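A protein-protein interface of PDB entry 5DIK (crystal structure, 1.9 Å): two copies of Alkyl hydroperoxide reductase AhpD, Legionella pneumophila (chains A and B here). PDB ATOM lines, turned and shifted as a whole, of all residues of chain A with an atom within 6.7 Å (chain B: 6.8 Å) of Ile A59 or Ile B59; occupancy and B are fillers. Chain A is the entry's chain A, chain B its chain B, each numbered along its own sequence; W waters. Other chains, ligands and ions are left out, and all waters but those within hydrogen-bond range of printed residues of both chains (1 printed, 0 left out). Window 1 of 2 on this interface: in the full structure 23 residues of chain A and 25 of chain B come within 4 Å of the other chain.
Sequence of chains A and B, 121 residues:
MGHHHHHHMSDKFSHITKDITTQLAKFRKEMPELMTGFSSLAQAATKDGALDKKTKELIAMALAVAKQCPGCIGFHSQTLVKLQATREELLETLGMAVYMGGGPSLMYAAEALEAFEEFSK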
ATOM      1  N   LEU A  51      19.922 -22.913  30.717  1.00  0.00           N
ATOM      2  CA  LEU A  51      20.115 -21.900  29.701  1.00  0.00           C
ATOM      3  C   LEU A  51      18.912 -21.925  28.795  1.00  0.00           C
ATOM      4  O   LEU A  51      18.457 -22.997  28.411  1.00  0.00           O
ATOM      5  CB  LEU A  51      21.407 -22.167  28.928  1.00  0.00           C
ATOM      6  CG  LEU A  51      22.682 -22.227  29.793  1.00  0.00           C
ATOM      7  CD1 LEU A  51      23.875 -22.502  28.906  1.00  0.00           C
ATOM      8  CD2 LEU A  51      22.900 -20.961  30.595  1.00  0.00           C
ATOM      9  N   LYS A  54      17.437 -19.287  23.372  1.00  0.00           N
ATOM     10  CA  LYS A  54      18.140 -18.158  22.739  1.00  0.00           C
ATOM     11  C   LYS A  54      19.617 -18.109  23.156  1.00  0.00           C
ATOM     12  O   LYS A  54      20.496 -17.886  22.332  1.00  0.00           O
ATOM     13  CB  LYS A  54      17.462 -16.834  23.108  1.00  0.00           C
ATOM     14  CG  LYS A  54      18.135 -15.599  22.518  1.00  0.00           C
ATOM     15  CD  LYS A  54      17.496 -14.333  23.072  1.00  0.00           C
ATOM     16  CE  LYS A  54      17.949 -14.059  24.494  1.00  0.00           C
ATOM     17  NZ  LYS A  54      17.101 -12.990  25.068  1.00  0.00           N
ATOM     18  N   THR A  55      19.875 -18.292  24.439  1.00  0.00           N
ATOM     19  CA  THR A  55      21.239 -18.321  24.951  1.00  0.00           C
ATOM     20  C   THR A  55      22.045 -19.440  24.305  1.00  0.00           C
ATOM     21  O   THR A  55      23.202 -19.222  23.944  1.00  0.00           O
ATOM     22  CB  THR A  55      21.278 -18.452  26.482  1.00  0.00           C
ATOM     23  OG1 THR A  55      20.605 -17.336  27.058  1.00  0.00           O
ATOM     24  CG2 THR A  55      22.709 -18.470  27.024  1.00  0.00           C
ATOM     25  N   LYS A  56      21.457 -20.646  24.228  1.00  0.00           N
ATOM     26  CA  LYS A  56      22.089 -21.769  23.559  1.00  0.00           C
ATOM     27  C   LYS A  56      22.374 -21.480  22.097  1.00  0.00           C
ATOM     28  O   LYS A  56      23.453 -21.833  21.593  1.00  0.00           O
ATOM     29  CB  LYS A  56      21.279 -23.057  23.709  1.00  0.00           C
ATOM     30  CG  LYS A  56      21.323 -23.577  25.123  1.00  0.00           C
ATOM     31  CD  LYS A  56      20.659 -24.922  25.232  1.00  0.00           C
ATOM     32  CE  LYS A  56      20.553 -25.321  26.693  1.00  0.00           C
ATOM     33  NZ  LYS A  56      20.136 -26.719  26.785  1.00  0.00           N
ATOM     34  N   GLU A  57      21.476 -20.776  21.414  1.00  0.00           N
ATOM     35  CA  GLU A  57      21.765 -20.410  20.041  1.00  0.00           C
ATOM     36  C   GLU A  57      22.863 -19.372  19.885  1.00  0.00           C
ATOM     37  O   GLU A  57      23.529 -19.368  18.843  1.00  0.00           O
ATOM     38  CB  GLU A  57      20.533 -19.866  19.296  1.00  0.00           C
ATOM     39  CG  GLU A  57      19.627 -20.955  18.831  1.00  0.00           C
ATOM     40  CD  GLU A  57      20.261 -21.919  17.836  1.00  0.00           C
ATOM     41  OE1 GLU A  57      20.809 -21.511  16.796  1.00  0.00           O
ATOM     42  OE2 GLU A  57      20.093 -23.110  18.068  1.00  0.00           O
ATOM     43  N   LEU A  58      22.993 -18.457  20.849  1.00  0.00           N
ATOM     44  CA  LEU A  58      24.097 -17.531  20.867  1.00  0.00           C
ATOM     45  C   LEU A  58      25.419 -18.311  20.987  1.00  0.00           C
ATOM     46  O   LEU A  58      26.400 -17.986  20.308  1.00  0.00           O
ATOM     47  CB  LEU A  58      23.938 -16.488  21.974  1.00  0.00           C
ATOM     48  CG  LEU A  58      22.822 -15.471  21.719  1.00  0.00           C
ATOM     49  CD1 LEU A  58      22.542 -14.663  22.957  1.00  0.00           C
ATOM     50  CD2 LEU A  58      23.166 -14.555  20.547  1.00  0.00           C
ATOM     51  N   ILE A  59      25.436 -19.351  21.817  1.00  0.00           N
ATOM     52  CA  ILE A  59      26.600 -20.226  21.916  1.00  0.00           C
ATOM     53  C   ILE A  59      26.878 -20.917  20.584  1.00  0.00           C
ATOM     54  O   ILE A  59      28.027 -20.936  20.123  1.00  0.00           O
ATOM     55  CB  ILE A  59      26.429 -21.260  23.042  1.00  0.00           C
ATOM     56  CG1 ILE A  59      26.395 -20.539  24.395  1.00  0.00           C
ATOM     57  CG2 ILE A  59      27.543 -22.315  23.009  1.00  0.00           C
ATOM     58  CD1 ILE A  59      25.862 -21.426  25.508  1.00  0.00           C
ATOM     59  N   ALA A  60      25.838 -21.431  19.938  1.00  0.00           N
ATOM     60  CA  ALA A  60      25.990 -22.073  18.622  1.00  0.00           C
ATOM     61  C   ALA A  60      26.566 -21.094  17.598  1.00  0.00           C
ATOM     62  O   ALA A  60      27.415 -21.473  16.805  1.00  0.00           O
ATOM     63  CB  ALA A  60      24.673 -22.644  18.131  1.00  0.00           C
ATOM     64  N   MET A  61      26.121 -19.843  17.636  1.00  0.00           N
ATOM     65  CA  MET A  61      26.629 -18.816  16.687  1.00  0.00           C
ATOM     66  C   MET A  61      28.108 -18.529  16.920  1.00  0.00           C
ATOM     67  O   MET A  61      28.874 -18.456  15.966  1.00  0.00           O
ATOM     68  CB  MET A  61      25.839 -17.524  16.782  1.00  0.00           C
ATOM     69  CG  MET A  61      26.395 -16.418  15.873  1.00  0.00           C
ATOM     70  SD  MET A  61      26.457 -16.894  14.125  1.00  0.00           S
ATOM     71  CE  MET A  61      24.703 -16.653  13.870  1.00  0.00           C
ATOM     72  N   ALA A  62      28.509 -18.396  18.176  1.00  0.00           N
ATOM     73  CA  ALA A  62      29.927 -18.252  18.496  1.00  0.00           C
ATOM     74  C   ALA A  62      30.770 -19.392  17.957  1.00  0.00           C
ATOM     75  O   ALA A  62      31.832 -19.148  17.358  1.00  0.00           O
ATOM     76  CB  ALA A  62      30.147 -18.096  19.988  1.00  0.00           C
ATOM     77  N   LEU A  63      30.293 -20.619  18.142  1.00  0.00           N
ATOM     78  CA  LEU A  63      30.974 -21.811  17.660  1.00  0.00           C
ATOM     79  C   LEU A  63      31.027 -21.866  16.131  1.00  0.00           C
ATOM     80  O   LEU A  63      32.030 -22.263  15.548  1.00  0.00           O
ATOM     81  CB  LEU A  63      30.253 -23.072  18.189  1.00  0.00           C
ATOM     82  CG  LEU A  63      30.444 -23.351  19.664  1.00  0.00           C
ATOM     83  CD1 LEU A  63      29.412 -24.339  20.197  1.00  0.00           C
ATOM     84  CD2 LEU A  63      31.813 -23.924  19.886  1.00  0.00           C
ATOM     85  N   ALA A  64      29.936 -21.464  15.488  1.00  0.00           N
ATOM     86  CA  ALA A  64      29.907 -21.379  14.033  1.00  0.00           C
ATOM     87  C   ALA A  64      30.932 -20.416  13.444  1.00  0.00           C
ATOM     88  O   ALA A  64      31.519 -20.702  12.391  1.00  0.00           O
ATOM     89  CB  ALA A  64      28.495 -21.024  13.554  1.00  0.00           C
ATOM     90  N   LEU A  80      18.384 -17.425  15.384  1.00  0.00           N
ATOM     91  CA  LEU A  80      18.478 -16.307  16.331  1.00  0.00           C
ATOM     92  C   LEU A  80      17.378 -15.258  16.062  1.00  0.00           C
ATOM     93  O   LEU A  80      16.782 -14.723  16.997  1.00  0.00           O
ATOM     94  CB  LEU A  80      19.824 -15.629  16.263  1.00  0.00           C
ATOM     95  CG  LEU A  80      20.982 -16.359  16.941  1.00  0.00           C
ATOM     96  CD1 LEU A  80      22.242 -15.568  16.645  1.00  0.00           C
ATOM     97  CD2 LEU A  80      20.794 -16.515  18.430  1.00  0.00           C
ATOM     98  N   GLU A  89      22.892  -8.491  21.537  1.00  0.00           N
ATOM     99  CA  GLU A  89      23.249  -9.840  22.035  1.00  0.00           C
ATOM    100  C   GLU A  89      24.138 -10.531  21.000  1.00  0.00           C
ATOM    101  O   GLU A  89      25.135 -11.151  21.366  1.00  0.00           O
ATOM    102  CB  GLU A  89      21.993 -10.693  22.326  1.00  0.00           C
ATOM    103  CG  GLU A  89      21.213 -10.199  23.526  1.00  0.00           C
ATOM    104  CD  GLU A  89      19.812 -10.798  23.645  1.00  0.00           C
ATOM    105  OE1 GLU A  89      19.172 -11.146  22.621  1.00  0.00           O
ATOM    106  OE2 GLU A  89      19.354 -10.926  24.785  1.00  0.00           O
ATOM    107  N   GLU A  92      27.697  -9.015  20.978  1.00  0.00           N
ATOM    108  CA  GLU A  92      28.485  -9.370  22.139  1.00  0.00           C
ATOM    109  C   GLU A  92      28.991 -10.807  22.047  1.00  0.00           C
ATOM    110  O   GLU A  92      30.104 -11.109  22.498  1.00  0.00           O
ATOM    111  CB  GLU A  92      27.726  -9.097  23.432  1.00  0.00           C
ATOM    112  CG  GLU A  92      27.567  -7.572  23.625  1.00  0.00           C
ATOM    113  CD  GLU A  92      27.055  -7.142  24.978  1.00  0.00           C
ATOM    114  OE1 GLU A  92      27.067  -7.982  25.927  1.00  0.00           O
ATOM    115  OE2 GLU A  92      26.627  -5.947  25.086  1.00  0.00           O
ATOM    116  N   THR A  93      28.185 -11.659  21.447  1.00  0.00           N
ATOM    117  CA  THR A  93      28.603 -13.022  21.211  1.00  0.00           C
ATOM    118  C   THR A  93      29.748 -13.072  20.203  1.00  0.00           C
ATOM    119  O   THR A  93      30.735 -13.799  20.381  1.00  0.00           O
ATOM    120  CB  THR A  93      27.429 -13.875  20.760  1.00  0.00           C
ATOM    121  OG1 THR A  93      26.368 -13.751  21.726  1.00  0.00           O
ATOM    122  CG2 THR A  93      27.841 -15.299  20.708  1.00  0.00           C
ATOM    123  N   MET A  96      33.037 -12.177  21.761  1.00  0.00           N
ATOM    124  CA  MET A  96      33.694 -13.309  22.427  1.00  0.00           C
ATOM    125  C   MET A  96      34.450 -14.208  21.430  1.00  0.00           C
ATOM    126  O   MET A  96      35.563 -14.646  21.706  1.00  0.00           O
ATOM    127  CB  MET A  96      32.684 -14.128  23.236  1.00  0.00           C
ATOM    128  CG  MET A  96      32.190 -13.416  24.478  1.00  0.00           C
ATOM    129  SD  MET A  96      33.510 -12.883  25.575  1.00  0.00           S
ATOM    130  CE  MET A  96      34.216 -14.491  26.024  1.00  0.00           C
ATOM    131  N   ALA A  97      33.868 -14.430  20.260  1.00  0.00           N
ATOM    132  CA  ALA A  97      34.524 -15.200  19.208  1.00  0.00           C
ATOM    133  C   ALA A  97      35.826 -14.521  18.766  1.00  0.00           C
ATOM    134  O   ALA A  97      36.828 -15.197  18.556  1.00  0.00           O
ATOM    135  CB  ALA A  97      33.584 -15.374  18.017  1.00  0.00           C
ATOM    136  N   MET A 100      38.538 -14.984  21.283  1.00  0.00           N
ATOM    137  CA  MET A 100      39.057 -16.371  21.260  1.00  0.00           C
ATOM    138  C   MET A 100      39.535 -16.848  19.886  1.00  0.00           C
ATOM    139  O   MET A 100      39.795 -18.029  19.702  1.00  0.00           O
ATOM    140  CB  MET A 100      37.965 -17.329  21.752  1.00  0.00           C
ATOM    141  CG  MET A 100      37.526 -17.015  23.158  1.00  0.00           C
ATOM    142  SD  MET A 100      38.823 -17.577  24.228  1.00  0.00           S
ATOM    143  CE  MET A 100      38.473 -19.362  24.169  1.00  0.00           C
ATOM    144  N   LEU B  51      24.833  -9.024  27.387  1.00  0.00           N
ATOM    145  CA  LEU B  51      25.030 -10.330  28.006  1.00  0.00           C
ATOM    146  C   LEU B  51      25.810 -10.104  29.282  1.00  0.00           C
ATOM    147  O   LEU B  51      26.733  -9.313  29.295  1.00  0.00           O
ATOM    148  CB  LEU B  51      25.784 -11.271  27.049  1.00  0.00           C
ATOM    149  CG  LEU B  51      25.089 -11.561  25.705  1.00  0.00           C
ATOM    150  CD1 LEU B  51      25.962 -12.462  24.856  1.00  0.00           C
ATOM    151  CD2 LEU B  51      23.714 -12.188  25.894  1.00  0.00           C
ATOM    152  N   LYS B  54      28.922 -13.803  33.310  1.00  0.00           N
ATOM    153  CA  LYS B  54      28.814 -15.264  33.420  1.00  0.00           C
ATOM    154  C   LYS B  54      28.406 -15.912  32.087  1.00  0.00           C
ATOM    155  O   LYS B  54      28.993 -16.923  31.681  1.00  0.00           O
ATOM    156  CB  LYS B  54      27.822 -15.637  34.510  1.00  0.00           C
ATOM    157  CG  LYS B  54      27.647 -17.150  34.689  1.00  0.00           C
ATOM    158  CD  LYS B  54      26.521 -17.424  35.669  1.00  0.00           C
ATOM    159  CE  LYS B  54      25.167 -17.186  35.012  1.00  0.00           C
ATOM    160  NZ  LYS B  54      24.127 -17.219  36.068  1.00  0.00           N
ATOM    161  N   THR B  55      27.429 -15.315  31.415  1.00  0.00           N
ATOM    162  CA  THR B  55      26.978 -15.797  30.117  1.00  0.00           C
ATOM    163  C   THR B  55      28.109 -15.764  29.093  1.00  0.00           C
ATOM    164  O   THR B  55      28.303 -16.718  28.362  1.00  0.00           O
ATOM    165  CB  THR B  55      25.786 -14.993  29.586  1.00  0.00           C
ATOM    166  OG1 THR B  55      24.710 -15.115  30.499  1.00  0.00           O
ATOM    167  CG2 THR B  55      25.336 -15.523  28.242  1.00  0.00           C
ATOM    168  N   LYS B  56      28.850 -14.654  29.055  1.00  0.00           N
ATOM    169  CA  LYS B  56      30.012 -14.535  28.169  1.00  0.00           C
ATOM    170  C   LYS B  56      31.074 -15.582  28.499  1.00  0.00           C
ATOM    171  O   LYS B  56      31.685 -16.133  27.590  1.00  0.00           O
ATOM    172  CB  LYS B  56      30.612 -13.128  28.229  1.00  0.00           C
ATOM    173  CG  LYS B  56      29.703 -12.120  27.562  1.00  0.00           C
ATOM    174  CD  LYS B  56      30.358 -10.749  27.520  1.00  0.00           C
ATOM    175  CE  LYS B  56      29.394  -9.726  27.046  1.00  0.00           C
ATOM    176  NZ  LYS B  56      30.125  -8.475  26.749  1.00  0.00           N
ATOM    177  N   GLU B  57      31.284 -15.889  29.766  1.00  0.00           N
ATOM    178  CA  GLU B  57      32.268 -16.937  30.112  1.00  0.00           C
ATOM    179  C   GLU B  57      31.825 -18.333  29.732  1.00  0.00           C
ATOM    180  O   GLU B  57      32.661 -19.174  29.447  1.00  0.00           O
ATOM    181  CB  GLU B  57      32.623 -16.971  31.593  1.00  0.00           C
ATOM    182  CG  GLU B  57      33.613 -15.928  31.987  1.00  0.00           C
ATOM    183  CD  GLU B  57      34.963 -16.085  31.311  1.00  0.00           C
ATOM    184  OE1 GLU B  57      35.592 -17.177  31.326  1.00  0.00           O
ATOM    185  OE2 GLU B  57      35.421 -15.065  30.833  1.00  0.00           O
ATOM    186  N   LEU B  58      30.528 -18.592  29.793  1.00  0.00           N
ATOM    187  CA  LEU B  58      29.980 -19.834  29.260  1.00  0.00           C
ATOM    188  C   LEU B  58      30.261 -19.971  27.779  1.00  0.00           C
ATOM    189  O   LEU B  58      30.620 -21.049  27.290  1.00  0.00           O
ATOM    190  CB  LEU B  58      28.476 -19.949  29.565  1.00  0.00           C
ATOM    191  CG  LEU B  58      28.170 -20.180  31.051  1.00  0.00           C
ATOM    192  CD1 LEU B  58      26.688 -20.007  31.316  1.00  0.00           C
ATOM    193  CD2 LEU B  58      28.630 -21.546  31.508  1.00  0.00           C
ATOM    194  N   ILE B  59      30.126 -18.872  27.043  1.00  0.00           N
ATOM    195  CA  ILE B  59      30.460 -18.859  25.615  1.00  0.00           C
ATOM    196  C   ILE B  59      31.955 -19.144  25.437  1.00  0.00           C
ATOM    197  O   ILE B  59      32.327 -19.957  24.612  1.00  0.00           O
ATOM    198  CB  ILE B  59      30.069 -17.537  24.963  1.00  0.00           C
ATOM    199  CG1 ILE B  59      28.542 -17.364  24.957  1.00  0.00           C
ATOM    200  CG2 ILE B  59      30.648 -17.397  23.562  1.00  0.00           C
ATOM    201  CD1 ILE B  59      28.116 -15.928  24.674  1.00  0.00           C
ATOM    202  N   ALA B  60      32.801 -18.474  26.230  1.00  0.00           N
ATOM    203  CA  ALA B  60      34.245 -18.730  26.204  1.00  0.00           C
ATOM    204  C   ALA B  60      34.576 -20.194  26.464  1.00  0.00           C
ATOM    205  O   ALA B  60      35.441 -20.755  25.798  1.00  0.00           O
ATOM    206  CB  ALA B  60      34.987 -17.838  27.184  1.00  0.00           C
ATOM    207  N   MET B  61      33.869 -20.817  27.409  1.00  0.00           N
ATOM    208  CA  MET B  61      34.110 -22.232  27.712  1.00  0.00           C
ATOM    209  C   MET B  61      33.732 -23.142  26.550  1.00  0.00           C
ATOM    210  O   MET B  61      34.485 -24.061  26.209  1.00  0.00           O
ATOM    211  CB  MET B  61      33.350 -22.671  28.974  1.00  0.00           C
ATOM    212  CG  MET B  61      33.499 -24.173  29.259  1.00  0.00           C
ATOM    213  SD  MET B  61      35.223 -24.687  29.497  1.00  0.00           S
ATOM    214  CE  MET B  61      35.351 -24.041  31.141  1.00  0.00           C
ATOM    215  N   ALA B  62      32.576 -22.880  25.905  1.00  0.00           N
ATOM    216  CA  ALA B  62      32.223 -23.609  24.700  1.00  0.00           C
ATOM    217  C   ALA B  62      33.287 -23.510  23.602  1.00  0.00           C
ATOM    218  O   ALA B  62      33.607 -24.515  22.977  1.00  0.00           O
ATOM    219  CB  ALA B  62      30.888 -23.146  24.147  1.00  0.00           C
ATOM    220  N   LEU B  63      33.777 -22.286  23.356  1.00  0.00           N
ATOM    221  CA  LEU B  63      34.827 -22.031  22.379  1.00  0.00           C
ATOM    222  C   LEU B  63      36.137 -22.737  22.761  1.00  0.00           C
ATOM    223  O   LEU B  63      36.829 -23.272  21.906  1.00  0.00           O
ATOM    224  CB  LEU B  63      35.096 -20.527  22.279  1.00  0.00           C
ATOM    225  CG  LEU B  63      34.003 -19.729  21.593  1.00  0.00           C
ATOM    226  CD1 LEU B  63      34.119 -18.239  21.880  1.00  0.00           C
ATOM    227  CD2 LEU B  63      34.098 -19.940  20.110  1.00  0.00           C
ATOM    228  N   ALA B  64      36.462 -22.756  24.040  1.00  0.00           N
ATOM    229  CA  ALA B  64      37.658 -23.489  24.514  1.00  0.00           C
ATOM    230  C   ALA B  64      37.614 -24.987  24.262  1.00  0.00           C
ATOM    231  O   ALA B  64      38.658 -25.613  23.949  1.00  0.00           O
ATOM    232  CB  ALA B  64      37.881 -23.230  26.002  1.00  0.00           C
ATOM    233  N   LEU B  80      34.649 -19.361  35.590  1.00  0.00           N
ATOM    234  CA  LEU B  80      33.239 -19.755  35.793  1.00  0.00           C
ATOM    235  C   LEU B  80      32.908 -20.020  37.271  1.00  0.00           C
ATOM    236  O   LEU B  80      31.831 -19.629  37.755  1.00  0.00           O
ATOM    237  CB  LEU B  80      32.888 -20.988  34.997  1.00  0.00           C
ATOM    238  CG  LEU B  80      32.695 -20.767  33.509  1.00  0.00           C
ATOM    239  CD1 LEU B  80      32.485 -22.155  32.893  1.00  0.00           C
ATOM    240  CD2 LEU B  80      31.515 -19.853  33.175  1.00  0.00           C
ATOM    241  N   GLU B  89      24.527 -25.147  34.323  1.00  0.00           N
ATOM    242  CA  GLU B  89      24.868 -24.197  33.257  1.00  0.00           C
ATOM    243  C   GLU B  89      26.097 -24.680  32.465  1.00  0.00           C
ATOM    244  O   GLU B  89      26.084 -24.638  31.242  1.00  0.00           O
ATOM    245  CB  GLU B  89      25.104 -22.791  33.791  1.00  0.00           C
ATOM    246  CG  GLU B  89      23.833 -22.130  34.328  1.00  0.00           C
ATOM    247  CD  GLU B  89      24.106 -20.885  35.166  1.00  0.00           C
ATOM    248  OE1 GLU B  89      25.154 -20.785  35.860  1.00  0.00           O
ATOM    249  OE2 GLU B  89      23.225 -20.013  35.173  1.00  0.00           O
ATOM    250  N   GLU B  92      25.105 -27.713  30.232  1.00  0.00           N
ATOM    251  CA  GLU B  92      24.303 -27.317  29.068  1.00  0.00           C
ATOM    252  C   GLU B  92      25.156 -26.642  27.980  1.00  0.00           C
ATOM    253  O   GLU B  92      24.927 -26.835  26.784  1.00  0.00           O
ATOM    254  CB  GLU B  92      23.122 -26.452  29.495  1.00  0.00           C
ATOM    255  CG  GLU B  92      22.127 -27.288  30.302  1.00  0.00           C
ATOM    256  CD  GLU B  92      20.858 -26.560  30.675  1.00  0.00           C
ATOM    257  OE1 GLU B  92      20.550 -25.528  30.017  1.00  0.00           O
ATOM    258  OE2 GLU B  92      20.166 -27.017  31.636  1.00  0.00           O
ATOM    259  N   THR B  93      26.149 -25.873  28.402  1.00  0.00           N
ATOM    260  CA  THR B  93      27.102 -25.286  27.484  1.00  0.00           C
ATOM    261  C   THR B  93      27.952 -26.364  26.797  1.00  0.00           C
ATOM    262  O   THR B  93      28.183 -26.307  25.587  1.00  0.00           O
ATOM    263  CB  THR B  93      27.994 -24.258  28.196  1.00  0.00           C
ATOM    264  OG1 THR B  93      27.145 -23.313  28.876  1.00  0.00           O
ATOM    265  CG2 THR B  93      28.803 -23.533  27.208  1.00  0.00           C
ATOM    266  N   LEU B  94      28.410 -27.354  27.569  1.00  0.00           N
ATOM    267  CA  LEU B  94      29.160 -28.467  26.983  1.00  0.00           C
ATOM    268  C   LEU B  94      28.332 -29.273  25.988  1.00  0.00           C
ATOM    269  O   LEU B  94      28.847 -29.714  24.948  1.00  0.00           O
ATOM    270  CB  LEU B  94      29.728 -29.373  28.082  1.00  0.00           C
ATOM    271  CG  LEU B  94      30.713 -28.638  29.024  1.00  0.00           C
ATOM    272  CD1 LEU B  94      31.195 -29.556  30.150  1.00  0.00           C
ATOM    273  CD2 LEU B  94      31.899 -28.078  28.265  1.00  0.00           C
ATOM    274  N   MET B  96      26.113 -28.086  23.968  1.00  0.00           N
ATOM    275  CA  MET B  96      26.132 -27.330  22.709  1.00  0.00           C
ATOM    276  C   MET B  96      27.451 -27.540  21.955  1.00  0.00           C
ATOM    277  O   MET B  96      27.451 -27.706  20.752  1.00  0.00           O
ATOM    278  CB  MET B  96      25.907 -25.849  22.971  1.00  0.00           C
ATOM    279  CG  MET B  96      24.468 -25.510  23.360  1.00  0.00           C
ATOM    280  SD  MET B  96      23.263 -26.026  22.126  1.00  0.00           S
ATOM    281  CE  MET B  96      23.750 -25.103  20.679  1.00  0.00           C
ATOM    282  N   ALA B  97      28.562 -27.597  22.683  1.00  0.00           N
ATOM    283  CA  ALA B  97      29.841 -27.904  22.090  1.00  0.00           C
ATOM    284  C   ALA B  97      29.834 -29.290  21.428  1.00  0.00           C
ATOM    285  O   ALA B  97      30.375 -29.452  20.328  1.00  0.00           O
ATOM    286  CB  ALA B  97      30.967 -27.826  23.125  1.00  0.00           C
ATOM    287  N   MET B 100      27.979 -29.255  18.175  1.00  0.00           N
ATOM    288  CA  MET B 100      28.713 -28.547  17.131  1.00  0.00           C
ATOM    289  C   MET B 100      30.119 -29.118  16.888  1.00  0.00           C
ATOM    290  O   MET B 100      30.891 -28.545  16.152  1.00  0.00           O
ATOM    291  CB  MET B 100      28.870 -27.065  17.513  1.00  0.00           C
ATOM    292  CG  MET B 100      27.533 -26.349  17.669  1.00  0.00           C
ATOM    293  SD  MET B 100      26.923 -26.102  16.026  1.00  0.00           S
ATOM    294  CE  MET B 100      27.937 -24.805  15.289  1.00  0.00           C
HETATM  295  O   HOH W   1      18.983 -28.246  28.744  1.00  0.00           O
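The backbone NH (N) of Leu A51 sits at hydrogen-bond distance from the side-chain carboxylate (OE1) of Glu B92, at 2.8 Å. The side-chain amino group (NZ) of Lys A56 lies within salt-bridge range of the side-chain carboxylate (OE1) of Glu B92 (3.5 Å). OE1 of Glu A92 sits at hydrogen-bond distance from N of Leu B51. OE1 of Glu A92 is in salt-bridge range of NZ of Lys B56 (3.2 Å).
OE2 of Glu A89 is in salt-bridge range of NZ of Lys A54 (3.1 Å). The backbone carbonyl oxygen of Glu A89 is in hydrogen-bond range of the side-chain hydroxyl of Thr A93 (2.9 Å). The side-chain amino group of Lys B54 lies within salt-bridge range of the side-chain carboxylate of Glu B89. O of Glu B89 is in hydrogen-bond range of OG1 of Thr B93 (2.9 Å).
CD1 of Leu A51 touches OG1 of Thr B93, 3.4 Å away. Lys A56 touches Met B96. CG1 of Ile B59 touches CG1 of Ile A59 (3.9 Å). Ala B62 touches Ile A59. Ile A59 touches Thr B93 (CD1 to CG2, 3.997 Å). Met B100 touches Ala A64 (CE to N, 3.9 Å). Leu B51 touches Glu A89. OG1 of Thr A93 touches CD1 of Leu B51 (3.4 Å). Met A96 touches Lys B56. CB of Ala B60 touches CE of Met A96, at 3.6 Å.
Printed residues of chain B within 4 Å of Ile A59: Ile B59, Ala B62, Thr B93 and Met B96. Of chain A, only Ile A59, Ala A62 and Met A96 come within 4 Å of Ile B59. Of the printed residues of chain A, Leu B58 touches Leu A51 (3.97 Å). Of the printed residues of chain A, Ala B64 touches Met A100 (3.9 Å). Of the printed residues of chain A, Glu B89 touches Leu A51. Of the printed residues of chain B, Ala A62 touches Ile B59 and Leu B63. Met A61 touches none of the printed residues of chain B. The nearest printed residue of chain A that does not touch Thr B93 is Leu A63 (5.9 Å).
Hydrophobic or aromatic side chains of chain B within 4 Å of the printed part of chain A: Leu B51, Leu B58, Ile B59, Ala B60, Ala B62, Leu B63, Met B96 and Met B100. Along chain B the printed residues that touch a printed residue of chain A span positions 51 to 100. Hydrophobic or aromatic side chains of chain A that line the printed part of chain B: Leu A51, Ile A59, Ala A60, Ala A62, Leu A63, Met A96 and Met A100. Among the printed residues, 29 pairs touch across the chains. Among the printed residues, Asp or Glu carboxylates within 4 Å of a Lys or Arg side-chain nitrogen of the other chain: Lys A56 with Glu B92 and Glu A92 with Lys B56.
Leu A51 touches Glu B89, and with the chains exchanged Glu A89 touches Leu B51. Ile A59 touches its own counterpart, Ile B59. Ile A59 touches Ala B62, and with the chains exchanged Ala A62 touches Ile B59. Ile A59 touches Thr B93, but with the chains exchanged Thr A93 does not touch Ile B59 (4.02 Å). 19 positions are printed for both chains. Of the 29 pairs that touch across the chains among the printed residues, 27 have their exchanged pair printed and touching as well.
Water W1 lies within hydrogen-bond range of the side-chain amino group (NZ) of Lys A56 (2.7 Å) and the side-chain carboxylate (OE2) of Glu B92 (3.4 Å).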
